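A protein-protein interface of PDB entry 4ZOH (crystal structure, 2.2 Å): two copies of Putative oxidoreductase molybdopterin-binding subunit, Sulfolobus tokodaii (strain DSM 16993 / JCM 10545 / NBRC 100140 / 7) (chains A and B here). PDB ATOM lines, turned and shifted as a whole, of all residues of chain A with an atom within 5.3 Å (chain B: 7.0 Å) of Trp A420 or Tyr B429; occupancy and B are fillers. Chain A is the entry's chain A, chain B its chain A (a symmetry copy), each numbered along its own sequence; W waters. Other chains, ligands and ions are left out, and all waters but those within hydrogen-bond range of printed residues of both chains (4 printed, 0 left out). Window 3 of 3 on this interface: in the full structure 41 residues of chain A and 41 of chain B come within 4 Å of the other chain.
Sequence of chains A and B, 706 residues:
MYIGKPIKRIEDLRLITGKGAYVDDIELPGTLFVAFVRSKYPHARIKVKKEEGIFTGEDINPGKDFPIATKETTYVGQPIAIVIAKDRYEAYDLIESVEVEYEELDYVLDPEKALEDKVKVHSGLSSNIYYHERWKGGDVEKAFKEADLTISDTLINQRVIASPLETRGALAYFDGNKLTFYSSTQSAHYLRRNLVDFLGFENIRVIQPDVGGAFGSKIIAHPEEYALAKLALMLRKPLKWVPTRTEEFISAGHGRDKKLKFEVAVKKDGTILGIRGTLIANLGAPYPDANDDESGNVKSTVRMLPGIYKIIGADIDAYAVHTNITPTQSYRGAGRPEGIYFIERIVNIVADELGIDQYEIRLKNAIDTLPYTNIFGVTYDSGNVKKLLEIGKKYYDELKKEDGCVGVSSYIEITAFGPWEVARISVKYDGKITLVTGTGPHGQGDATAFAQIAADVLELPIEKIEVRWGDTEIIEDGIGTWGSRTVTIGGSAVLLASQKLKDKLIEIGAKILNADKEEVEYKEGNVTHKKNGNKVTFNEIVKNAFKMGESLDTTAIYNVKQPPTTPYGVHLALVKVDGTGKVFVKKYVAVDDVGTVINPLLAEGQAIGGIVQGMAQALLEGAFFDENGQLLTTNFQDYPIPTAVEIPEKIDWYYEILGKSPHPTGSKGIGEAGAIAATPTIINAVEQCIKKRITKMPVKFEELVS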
ATOM      1  N   ARG A 193     -17.240 -10.771 -23.510  1.00  0.00           N
ATOM      2  CA  ARG A 193     -17.219 -10.396 -24.906  1.00  0.00           C
ATOM      3  C   ARG A 193     -18.567  -9.831 -25.340  1.00  0.00           C
ATOM      4  O   ARG A 193     -18.600  -8.846 -26.055  1.00  0.00           O
ATOM      5  CB  ARG A 193     -16.796 -11.534 -25.774  1.00  0.00           C
ATOM      6  CG  ARG A 193     -15.317 -11.748 -25.780  1.00  0.00           C
ATOM      7  CD  ARG A 193     -14.926 -12.828 -26.798  1.00  0.00           C
ATOM      8  NE  ARG A 193     -15.433 -14.184 -26.436  1.00  0.00           N
ATOM      9  CZ  ARG A 193     -14.835 -15.027 -25.566  1.00  0.00           C
ATOM     10  NH1 ARG A 193     -13.750 -14.680 -24.881  1.00  0.00           N
ATOM     11  NH2 ARG A 193     -15.341 -16.234 -25.365  1.00  0.00           N
ATOM     12  N   GLY A 418     -14.713 -26.311 -31.062  1.00  0.00           N
ATOM     13  CA  GLY A 418     -13.627 -25.352 -30.839  1.00  0.00           C
ATOM     14  C   GLY A 418     -14.168 -24.009 -30.367  1.00  0.00           C
ATOM     15  O   GLY A 418     -15.341 -23.941 -29.901  1.00  0.00           O
ATOM     16  N   PRO A 419     -13.391 -22.924 -30.571  1.00  0.00           N
ATOM     17  CA  PRO A 419     -12.216 -22.938 -31.446  1.00  0.00           C
ATOM     18  C   PRO A 419     -10.978 -23.202 -30.663  1.00  0.00           C
ATOM     19  O   PRO A 419      -9.921 -23.581 -31.211  1.00  0.00           O
ATOM     20  CB  PRO A 419     -12.206 -21.483 -32.029  1.00  0.00           C
ATOM     21  CG  PRO A 419     -12.772 -20.671 -30.862  1.00  0.00           C
ATOM     22  CD  PRO A 419     -13.939 -21.548 -30.432  1.00  0.00           C
ATOM     23  N   TRP A 420     -11.063 -22.992 -29.359  1.00  0.00           N
ATOM     24  CA  TRP A 420      -9.838 -23.147 -28.552  1.00  0.00           C
ATOM     25  C   TRP A 420     -10.268 -23.219 -27.096  1.00  0.00           C
ATOM     26  O   TRP A 420     -11.457 -23.041 -26.778  1.00  0.00           O
ATOM     27  CB  TRP A 420      -8.798 -21.996 -28.815  1.00  0.00           C
ATOM     28  CG  TRP A 420      -9.341 -20.634 -28.969  1.00  0.00           C
ATOM     29  CD1 TRP A 420      -9.572 -19.958 -30.181  1.00  0.00           C
ATOM     30  CD2 TRP A 420      -9.715 -19.709 -27.927  1.00  0.00           C
ATOM     31  NE1 TRP A 420     -10.124 -18.715 -29.928  1.00  0.00           N
ATOM     32  CE2 TRP A 420     -10.181 -18.506 -28.569  1.00  0.00           C
ATOM     33  CE3 TRP A 420      -9.649 -19.741 -26.522  1.00  0.00           C
ATOM     34  CZ2 TRP A 420     -10.653 -17.380 -27.842  1.00  0.00           C
ATOM     35  CZ3 TRP A 420     -10.138 -18.619 -25.796  1.00  0.00           C
ATOM     36  CH2 TRP A 420     -10.588 -17.430 -26.467  1.00  0.00           C
ATOM     37  N   GLU A 421      -9.337 -23.489 -26.206  1.00  0.00           N
ATOM     38  CA  GLU A 421      -9.694 -23.343 -24.775  1.00  0.00           C
ATOM     39  C   GLU A 421      -8.434 -23.068 -24.018  1.00  0.00           C
ATOM     40  O   GLU A 421      -7.350 -23.375 -24.539  1.00  0.00           O
ATOM     41  CB  GLU A 421     -10.554 -24.528 -24.238  1.00  0.00           C
ATOM     42  CG  GLU A 421     -11.036 -24.316 -22.796  1.00  0.00           C
ATOM     43  CD  GLU A 421     -11.813 -23.018 -22.707  1.00  0.00           C
ATOM     44  OE1 GLU A 421     -13.029 -23.012 -23.038  1.00  0.00           O
ATOM     45  OE2 GLU A 421     -11.152 -22.019 -22.357  1.00  0.00           O
ATOM     46  N   VAL A 422      -8.529 -22.504 -22.803  1.00  0.00           N
ATOM     47  CA  VAL A 422      -7.338 -22.028 -22.108  1.00  0.00           C
ATOM     48  C   VAL A 422      -7.125 -22.722 -20.764  1.00  0.00           C
ATOM     49  O   VAL A 422      -8.064 -23.158 -20.125  1.00  0.00           O
ATOM     50  CB  VAL A 422      -7.452 -20.461 -21.937  1.00  0.00           C
ATOM     51  CG1 VAL A 422      -6.172 -19.847 -21.450  1.00  0.00           C
ATOM     52  CG2 VAL A 422      -7.924 -19.796 -23.258  1.00  0.00           C
ATOM     53  N   ASP A 477      -8.209 -15.868 -20.833  1.00  0.00           N
ATOM     54  CA  ASP A 477      -9.437 -15.881 -21.587  1.00  0.00           C
ATOM     55  C   ASP A 477     -10.043 -17.279 -21.511  1.00  0.00           C
ATOM     56  O   ASP A 477      -9.556 -18.146 -20.789  1.00  0.00           O
ATOM     57  CB  ASP A 477      -9.215 -15.465 -23.088  1.00  0.00           C
ATOM     58  CG  ASP A 477     -10.360 -14.620 -23.637  1.00  0.00           C
ATOM     59  OD1 ASP A 477     -10.139 -13.560 -24.242  1.00  0.00           O
ATOM     60  OD2 ASP A 477     -11.516 -15.001 -23.476  1.00  0.00           O
ATOM     61  N   GLY A 478     -11.133 -17.477 -22.220  1.00  0.00           N
ATOM     62  CA  GLY A 478     -11.748 -18.794 -22.253  1.00  0.00           C
ATOM     63  C   GLY A 478     -12.869 -18.798 -23.240  1.00  0.00           C
ATOM     64  O   GLY A 478     -13.347 -17.732 -23.697  1.00  0.00           O
ATOM     65  N   ILE A 479     -13.316 -20.013 -23.547  1.00  0.00           N
ATOM     66  CA  ILE A 479     -14.508 -20.147 -24.325  1.00  0.00           C
ATOM     67  C   ILE A 479     -15.737 -20.397 -23.467  1.00  0.00           C
ATOM     68  O   ILE A 479     -16.628 -19.534 -23.423  1.00  0.00           O
ATOM     69  CB  ILE A 479     -14.325 -21.118 -25.559  1.00  0.00           C
ATOM     70  CG1 ILE A 479     -13.352 -20.458 -26.562  1.00  0.00           C
ATOM     71  CG2 ILE A 479     -15.697 -21.486 -26.180  1.00  0.00           C
ATOM     72  CD1 ILE A 479     -13.965 -19.271 -27.356  1.00  0.00           C
ATOM     73  N   ARG A 485     -17.934 -30.145 -24.219  1.00  0.00           N
ATOM     74  CA  ARG A 485     -16.588 -29.841 -24.662  1.00  0.00           C
ATOM     75  C   ARG A 485     -15.633 -29.723 -23.509  1.00  0.00           C
ATOM     76  O   ARG A 485     -14.427 -29.722 -23.705  1.00  0.00           O
ATOM     77  CB  ARG A 485     -16.591 -28.485 -25.476  1.00  0.00           C
ATOM     78  CG  ARG A 485     -16.740 -27.218 -24.592  1.00  0.00           C
ATOM     79  CD  ARG A 485     -17.045 -25.930 -25.422  1.00  0.00           C
ATOM     80  NE  ARG A 485     -15.915 -25.568 -26.274  1.00  0.00           N
ATOM     81  CZ  ARG A 485     -14.780 -25.004 -25.829  1.00  0.00           C
ATOM     82  NH1 ARG A 485     -14.679 -24.689 -24.537  1.00  0.00           N
ATOM     83  NH2 ARG A 485     -13.753 -24.734 -26.663  1.00  0.00           N
ATOM     84  N   ILE A 489     -11.880 -30.563 -24.526  1.00  0.00           N
ATOM     85  CA  ILE A 489     -11.120 -29.378 -24.984  1.00  0.00           C
ATOM     86  C   ILE A 489     -10.448 -28.638 -23.816  1.00  0.00           C
ATOM     87  O   ILE A 489      -9.222 -28.256 -23.848  1.00  0.00           O
ATOM     88  CB  ILE A 489     -12.040 -28.421 -25.776  1.00  0.00           C
ATOM     89  CG1 ILE A 489     -12.793 -29.162 -26.903  1.00  0.00           C
ATOM     90  CG2 ILE A 489     -11.191 -27.299 -26.375  1.00  0.00           C
ATOM     91  CD1 ILE A 489     -11.935 -30.078 -27.807  1.00  0.00           C
ATOM     92  N   ILE A 557      -2.943 -22.591 -24.638  1.00  0.00           N
ATOM     93  CA  ILE A 557      -4.196 -22.419 -25.327  1.00  0.00           C
ATOM     94  C   ILE A 557      -4.149 -23.647 -26.204  1.00  0.00           C
ATOM     95  O   ILE A 557      -3.149 -23.855 -26.932  1.00  0.00           O
ATOM     96  CB  ILE A 557      -4.241 -21.120 -26.167  1.00  0.00           C
ATOM     97  CG1 ILE A 557      -4.217 -19.859 -25.276  1.00  0.00           C
ATOM     98  CG2 ILE A 557      -5.433 -21.143 -27.127  1.00  0.00           C
ATOM     99  CD1 ILE A 557      -4.008 -18.532 -26.039  1.00  0.00           C
ATOM    100  N   TYR A 558      -5.202 -24.448 -26.119  1.00  0.00           N
ATOM    101  CA  TYR A 558      -5.378 -25.592 -26.994  1.00  0.00           C
ATOM    102  C   TYR A 558      -6.325 -25.205 -28.130  1.00  0.00           C
ATOM    103  O   TYR A 558      -7.520 -25.072 -27.933  1.00  0.00           O
ATOM    104  CB  TYR A 558      -5.895 -26.824 -26.175  1.00  0.00           C
ATOM    105  CG  TYR A 558      -6.145 -28.061 -27.028  1.00  0.00           C
ATOM    106  CD1 TYR A 558      -5.057 -28.772 -27.628  1.00  0.00           C
ATOM    107  CD2 TYR A 558      -7.444 -28.522 -27.254  1.00  0.00           C
ATOM    108  CE1 TYR A 558      -5.287 -29.911 -28.418  1.00  0.00           C
ATOM    109  CE2 TYR A 558      -7.670 -29.651 -28.067  1.00  0.00           C
ATOM    110  CZ  TYR A 558      -6.580 -30.332 -28.630  1.00  0.00           C
ATOM    111  OH  TYR A 558      -6.790 -31.422 -29.387  1.00  0.00           O
ATOM    112  N   ASN A 559      -5.762 -24.934 -29.303  1.00  0.00           N
ATOM    113  CA  ASN A 559      -6.554 -24.581 -30.494  1.00  0.00           C
ATOM    114  C   ASN A 559      -7.165 -25.882 -31.030  1.00  0.00           C
ATOM    115  O   ASN A 559      -6.532 -26.891 -31.024  1.00  0.00           O
ATOM    116  CB  ASN A 559      -5.707 -23.826 -31.542  1.00  0.00           C
ATOM    117  CG  ASN A 559      -4.362 -24.511 -31.808  1.00  0.00           C
ATOM    118  OD1 ASN A 559      -3.644 -24.899 -30.869  1.00  0.00           O
ATOM    119  ND2 ASN A 559      -3.998 -24.657 -33.095  1.00  0.00           N
ATOM    120  N   VAL A 560      -8.424 -25.878 -31.394  1.00  0.00           N
ATOM    121  CA  VAL A 560      -9.070 -27.144 -31.825  1.00  0.00           C
ATOM    122  C   VAL A 560      -8.980 -27.256 -33.366  1.00  0.00           C
ATOM    123  O   VAL A 560      -9.720 -26.585 -34.075  1.00  0.00           O
ATOM    124  CB  VAL A 560     -10.526 -27.223 -31.340  1.00  0.00           C
ATOM    125  CG1 VAL A 560     -11.271 -28.457 -31.917  1.00  0.00           C
ATOM    126  CG2 VAL A 560     -10.585 -27.185 -29.794  1.00  0.00           C
ATOM    127  N   VAL B 427      -3.181 -10.470 -22.540  1.00  0.00           N
ATOM    128  CA  VAL B 427      -4.032  -9.849 -23.569  1.00  0.00           C
ATOM    129  C   VAL B 427      -5.177 -10.745 -23.936  1.00  0.00           C
ATOM    130  O   VAL B 427      -4.964 -11.927 -24.278  1.00  0.00           O
ATOM    131  CB  VAL B 427      -3.217  -9.504 -24.861  1.00  0.00           C
ATOM    132  CG1 VAL B 427      -4.099  -8.810 -25.906  1.00  0.00           C
ATOM    133  CG2 VAL B 427      -1.973  -8.676 -24.482  1.00  0.00           C
ATOM    134  N   LYS B 428      -6.404 -10.208 -23.887  1.00  0.00           N
ATOM    135  CA  LYS B 428      -7.591 -11.065 -24.107  1.00  0.00           C
ATOM    136  C   LYS B 428      -7.835 -11.114 -25.663  1.00  0.00           C
ATOM    137  O   LYS B 428      -7.263 -10.315 -26.420  1.00  0.00           O
ATOM    138  CB  LYS B 428      -8.808 -10.503 -23.390  1.00  0.00           C
ATOM    139  CG  LYS B 428      -8.651 -10.358 -21.864  1.00  0.00           C
ATOM    140  CD  LYS B 428      -9.972 -10.211 -21.117  1.00  0.00           C
ATOM    141  CE  LYS B 428      -9.766 -10.484 -19.586  1.00  0.00           C
ATOM    142  NZ  LYS B 428      -9.374 -11.918 -19.368  1.00  0.00           N
ATOM    143  N   TYR B 429      -8.660 -12.028 -26.120  1.00  0.00           N
ATOM    144  CA  TYR B 429      -8.937 -12.185 -27.544  1.00  0.00           C
ATOM    145  C   TYR B 429      -9.372 -10.900 -28.209  1.00  0.00           C
ATOM    146  O   TYR B 429      -8.952 -10.689 -29.363  1.00  0.00           O
ATOM    147  CB  TYR B 429     -10.037 -13.208 -27.735  1.00  0.00           C
ATOM    148  CG  TYR B 429     -10.316 -13.607 -29.165  1.00  0.00           C
ATOM    149  CD1 TYR B 429      -9.467 -14.482 -29.880  1.00  0.00           C
ATOM    150  CD2 TYR B 429     -11.473 -13.150 -29.802  1.00  0.00           C
ATOM    151  CE1 TYR B 429      -9.795 -14.862 -31.189  1.00  0.00           C
ATOM    152  CE2 TYR B 429     -11.774 -13.500 -31.123  1.00  0.00           C
ATOM    153  CZ  TYR B 429     -10.965 -14.377 -31.795  1.00  0.00           C
ATOM    154  OH  TYR B 429     -11.339 -14.714 -33.084  1.00  0.00           O
ATOM    155  N   ASP B 430     -10.222 -10.089 -27.509  1.00  0.00           N
ATOM    156  CA  ASP B 430     -10.763  -8.821 -28.071  1.00  0.00           C
ATOM    157  C   ASP B 430      -9.644  -7.766 -28.087  1.00  0.00           C
ATOM    158  O   ASP B 430      -9.805  -6.716 -28.696  1.00  0.00           O
ATOM    159  CB  ASP B 430     -11.984  -8.332 -27.303  1.00  0.00           C
ATOM    160  CG  ASP B 430     -11.716  -8.321 -25.742  1.00  0.00           C
ATOM    161  OD1 ASP B 430     -11.637  -9.410 -25.100  1.00  0.00           O
ATOM    162  OD2 ASP B 430     -11.496  -7.233 -25.212  1.00  0.00           O
ATOM    163  N   GLY B 431      -8.524  -8.048 -27.415  1.00  0.00           N
ATOM    164  CA  GLY B 431      -7.398  -7.108 -27.389  1.00  0.00           C
ATOM    165  C   GLY B 431      -7.086  -6.429 -26.061  1.00  0.00           C
ATOM    166  O   GLY B 431      -6.036  -5.752 -25.926  1.00  0.00           O
ATOM    167  N   LYS B 432      -7.948  -6.612 -25.068  1.00  0.00           N
ATOM    168  CA  LYS B 432      -7.787  -5.880 -23.795  1.00  0.00           C
ATOM    169  C   LYS B 432      -6.486  -6.239 -23.094  1.00  0.00           C
ATOM    170  O   LYS B 432      -6.154  -7.384 -22.988  1.00  0.00           O
ATOM    171  CB  LYS B 432      -8.940  -6.105 -22.853  1.00  0.00           C
ATOM    172  CG  LYS B 432      -8.795  -5.295 -21.544  1.00  0.00           C
ATOM    173  CD  LYS B 432      -9.563  -5.946 -20.386  1.00  0.00           C
ATOM    174  CE  LYS B 432      -9.661  -5.036 -19.168  1.00  0.00           C
ATOM    175  NZ  LYS B 432      -8.349  -4.590 -18.649  1.00  0.00           N
ATOM    176  N   ASN B 539      -4.925  -5.952 -33.068  1.00  0.00           N
ATOM    177  CA  ASN B 539      -6.047  -6.828 -32.882  1.00  0.00           C
ATOM    178  C   ASN B 539      -6.003  -8.128 -33.744  1.00  0.00           C
ATOM    179  O   ASN B 539      -6.348  -9.210 -33.236  1.00  0.00           O
ATOM    180  CB  ASN B 539      -7.373  -6.074 -33.031  1.00  0.00           C
ATOM    181  CG  ASN B 539      -7.632  -5.119 -31.857  1.00  0.00           C
ATOM    182  OD1 ASN B 539      -7.314  -3.902 -31.911  1.00  0.00           O
ATOM    183  ND2 ASN B 539      -8.223  -5.655 -30.786  1.00  0.00           N
ATOM    184  N   VAL B 542      -3.470 -10.559 -32.227  1.00  0.00           N
ATOM    185  CA  VAL B 542      -3.989 -11.114 -30.987  1.00  0.00           C
ATOM    186  C   VAL B 542      -4.950 -12.248 -31.367  1.00  0.00           C
ATOM    187  O   VAL B 542      -4.798 -13.361 -30.902  1.00  0.00           O
ATOM    188  CB  VAL B 542      -4.683 -10.044 -30.150  1.00  0.00           C
ATOM    189  CG1 VAL B 542      -5.486 -10.702 -29.010  1.00  0.00           C
ATOM    190  CG2 VAL B 542      -3.677  -9.042 -29.583  1.00  0.00           C
ATOM    191  N   LYS B 543      -5.929 -11.997 -32.235  1.00  0.00           N
ATOM    192  CA  LYS B 543      -6.851 -13.109 -32.635  1.00  0.00           C
ATOM    193  C   LYS B 543      -6.180 -14.337 -33.261  1.00  0.00           C
ATOM    194  O   LYS B 543      -6.536 -15.512 -32.976  1.00  0.00           O
ATOM    195  CB  LYS B 543      -7.945 -12.590 -33.486  1.00  0.00           C
ATOM    196  CG  LYS B 543      -8.651 -11.491 -32.763  1.00  0.00           C
ATOM    197  CD  LYS B 543      -9.890 -11.149 -33.515  1.00  0.00           C
ATOM    198  CE  LYS B 543     -10.651 -10.052 -32.788  1.00  0.00           C
ATOM    199  NZ  LYS B 543     -12.048 -10.354 -33.114  1.00  0.00           N
ATOM    200  N   ASN B 544      -5.176 -14.055 -34.076  1.00  0.00           N
ATOM    201  CA  ASN B 544      -4.350 -15.088 -34.651  1.00  0.00           C
ATOM    202  C   ASN B 544      -3.481 -15.789 -33.628  1.00  0.00           C
ATOM    203  O   ASN B 544      -3.237 -16.964 -33.777  1.00  0.00           O
ATOM    204  CB  ASN B 544      -3.577 -14.578 -35.901  1.00  0.00           C
ATOM    205  CG  ASN B 544      -4.518 -14.417 -37.106  1.00  0.00           C
ATOM    206  OD1 ASN B 544      -4.948 -15.418 -37.709  1.00  0.00           O
ATOM    207  ND2 ASN B 544      -4.928 -13.164 -37.400  1.00  0.00           N
ATOM    208  N   ALA B 545      -3.025 -15.102 -32.586  1.00  0.00           N
ATOM    209  CA  ALA B 545      -2.291 -15.825 -31.533  1.00  0.00           C
ATOM    210  C   ALA B 545      -3.145 -16.913 -30.863  1.00  0.00           C
ATOM    211  O   ALA B 545      -2.657 -17.999 -30.582  1.00  0.00           O
ATOM    212  CB  ALA B 545      -1.718 -14.866 -30.485  1.00  0.00           C
ATOM    213  N   PHE B 546      -4.419 -16.606 -30.620  1.00  0.00           N
ATOM    214  CA  PHE B 546      -5.324 -17.550 -30.047  1.00  0.00           C
ATOM    215  C   PHE B 546      -5.580 -18.729 -31.020  1.00  0.00           C
ATOM    216  O   PHE B 546      -5.483 -19.909 -30.624  1.00  0.00           O
ATOM    217  CB  PHE B 546      -6.625 -16.840 -29.646  1.00  0.00           C
ATOM    218  CG  PHE B 546      -6.578 -16.162 -28.286  1.00  0.00           C
ATOM    219  CD1 PHE B 546      -7.058 -16.841 -27.137  1.00  0.00           C
ATOM    220  CD2 PHE B 546      -6.110 -14.837 -28.130  1.00  0.00           C
ATOM    221  CE1 PHE B 546      -7.066 -16.233 -25.875  1.00  0.00           C
ATOM    222  CE2 PHE B 546      -6.119 -14.211 -26.862  1.00  0.00           C
ATOM    223  CZ  PHE B 546      -6.594 -14.919 -25.715  1.00  0.00           C
ATOM    224  N   LYS B 547      -5.857 -18.436 -32.287  1.00  0.00           N
ATOM    225  CA  LYS B 547      -6.077 -19.504 -33.317  1.00  0.00           C
ATOM    226  C   LYS B 547      -4.867 -20.433 -33.481  1.00  0.00           C
ATOM    227  O   LYS B 547      -5.024 -21.604 -33.713  1.00  0.00           O
ATOM    228  CB  LYS B 547      -6.438 -18.915 -34.679  1.00  0.00           C
ATOM    229  CG  LYS B 547      -7.915 -18.693 -34.906  1.00  0.00           C
ATOM    230  CD  LYS B 547      -8.129 -17.682 -36.037  1.00  0.00           C
ATOM    231  CE  LYS B 547      -9.221 -16.703 -35.635  1.00  0.00           C
ATOM    232  NZ  LYS B 547      -9.909 -16.063 -36.781  1.00  0.00           N
ATOM    233  N   MET B 548      -3.673 -19.887 -33.342  1.00  0.00           N
ATOM    234  CA  MET B 548      -2.440 -20.630 -33.420  1.00  0.00           C
ATOM    235  C   MET B 548      -2.043 -21.332 -32.112  1.00  0.00           C
ATOM    236  O   MET B 548      -0.932 -21.902 -32.024  1.00  0.00           O
ATOM    237  CB  MET B 548      -1.319 -19.676 -33.800  1.00  0.00           C
ATOM    238  CG  MET B 548      -1.301 -19.233 -35.265  1.00  0.00           C
ATOM    239  SD  MET B 548      -0.275 -17.750 -35.521  1.00  0.00           S
ATOM    240  CE  MET B 548       1.289 -18.242 -34.785  1.00  0.00           C
ATOM    241  N   GLY B 549      -2.922 -21.293 -31.101  1.00  0.00           N
ATOM    242  CA  GLY B 549      -2.617 -21.851 -29.743  1.00  0.00           C
ATOM    243  C   GLY B 549      -1.434 -21.175 -29.076  1.00  0.00           C
ATOM    244  O   GLY B 549      -0.675 -21.814 -28.404  1.00  0.00           O
HETATM  245  O   HOH W   1     -12.282 -12.090 -24.789  1.00  0.00           O
HETATM  246  O   HOH W   2      -0.146 -22.386 -25.624  1.00  0.00           O
HETATM  247  O   HOH W   3     -11.097 -17.824 -32.311  1.00  0.00           O
HETATM  248  O   HOH W   4      -1.039 -24.396 -34.157  1.00  0.00           O
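CD1 of Tyr B429 touches CZ2 of Trp A420, at 3.7 Å.
Trp A420 touches Phe B546.
CB of Lys B428 touches OD1 of Asp A477, at 3.4 Å.
CB of Asp A477 touches CE1 of Phe B546, 3.6 Å away.
CD1 of Ile A557 touches CD1 of Phe B546 (3.7 Å).
Ile A557 touches Gly B549.
C of Met B548 touches CG of Asn A559, 3.9 Å away.
OD1 of Asn A559 touches CA of Gly B549, 3.4 Å away.
No position is printed for both chains.
Of the 10 pairs that touch across the chains among the printed residues, none has its exchanged pair printed and touching as well.
Of chain B, only Tyr B429 (3.7 Å) and Phe B546 (3.6 Å) come within 4 Å of Trp A420.
Tyr B429 touches two residues of chain A.
Printed residues of chain A within 4 Å of Phe B546: Trp A420 (3.6 Å), Asp A477 (3.6 Å) and Ile A557 (3.7 Å).
Printed residues of chain A within 4 Å of Lys B547: Asn A559.
Printed residues of chain A within 4 Å of Gly B549: Ile A557 and Asn A559.
The nearest residue of chain B that does not touch Trp A420 is Lys B547 (4.5 Å).
The nearest printed residue of chain B that does not touch Ile A557 is Ala B545 (4.8 Å).
Along chain B the printed residues that touch a printed residue of chain A span positions 428 to 549.
Printed residues of chain A that touch a printed residue of chain B: Trp A420, Asp A477, Ile A557 and Asn A559.
Among the printed residues, 10 pairs touch across the chains.
The side-chain carboxylate of Asp A477 sits at hydrogen-bond distance from the backbone NH of Tyr B429.
The backbone carbonyl oxygen of Lys B547 sits close to the side-chain amide nitrogen of Asn A559 (3.3 Å).
NH1 of Arg A193 is in salt-bridge range of OD2 of Asp A477 (2.7 Å).
O of Trp A420 is in hydrogen-bond range of NH2 of Arg A485.
Water W1 lies within hydrogen-bond range of the side-chain carboxylate of Asp A477, the side-chain carboxylate of Asp B430 and the guanidinium group of Arg A193.
Water W3 bridges the indole nitrogen of Trp A420 (2.7 Å) and the side-chain hydroxyl of Tyr B429 (3.2 Å).
Water W2 lies within hydrogen-bond range of O of Gly B549 (2.9 Å) and N of Ile A557 (3.0 Å).
Water W4 bridges the side-chain amide nitrogen (ND2) of Asn A559 (3.2 Å) and the backbone carbonyl oxygen (O) of Met B548 (3.3 Å).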
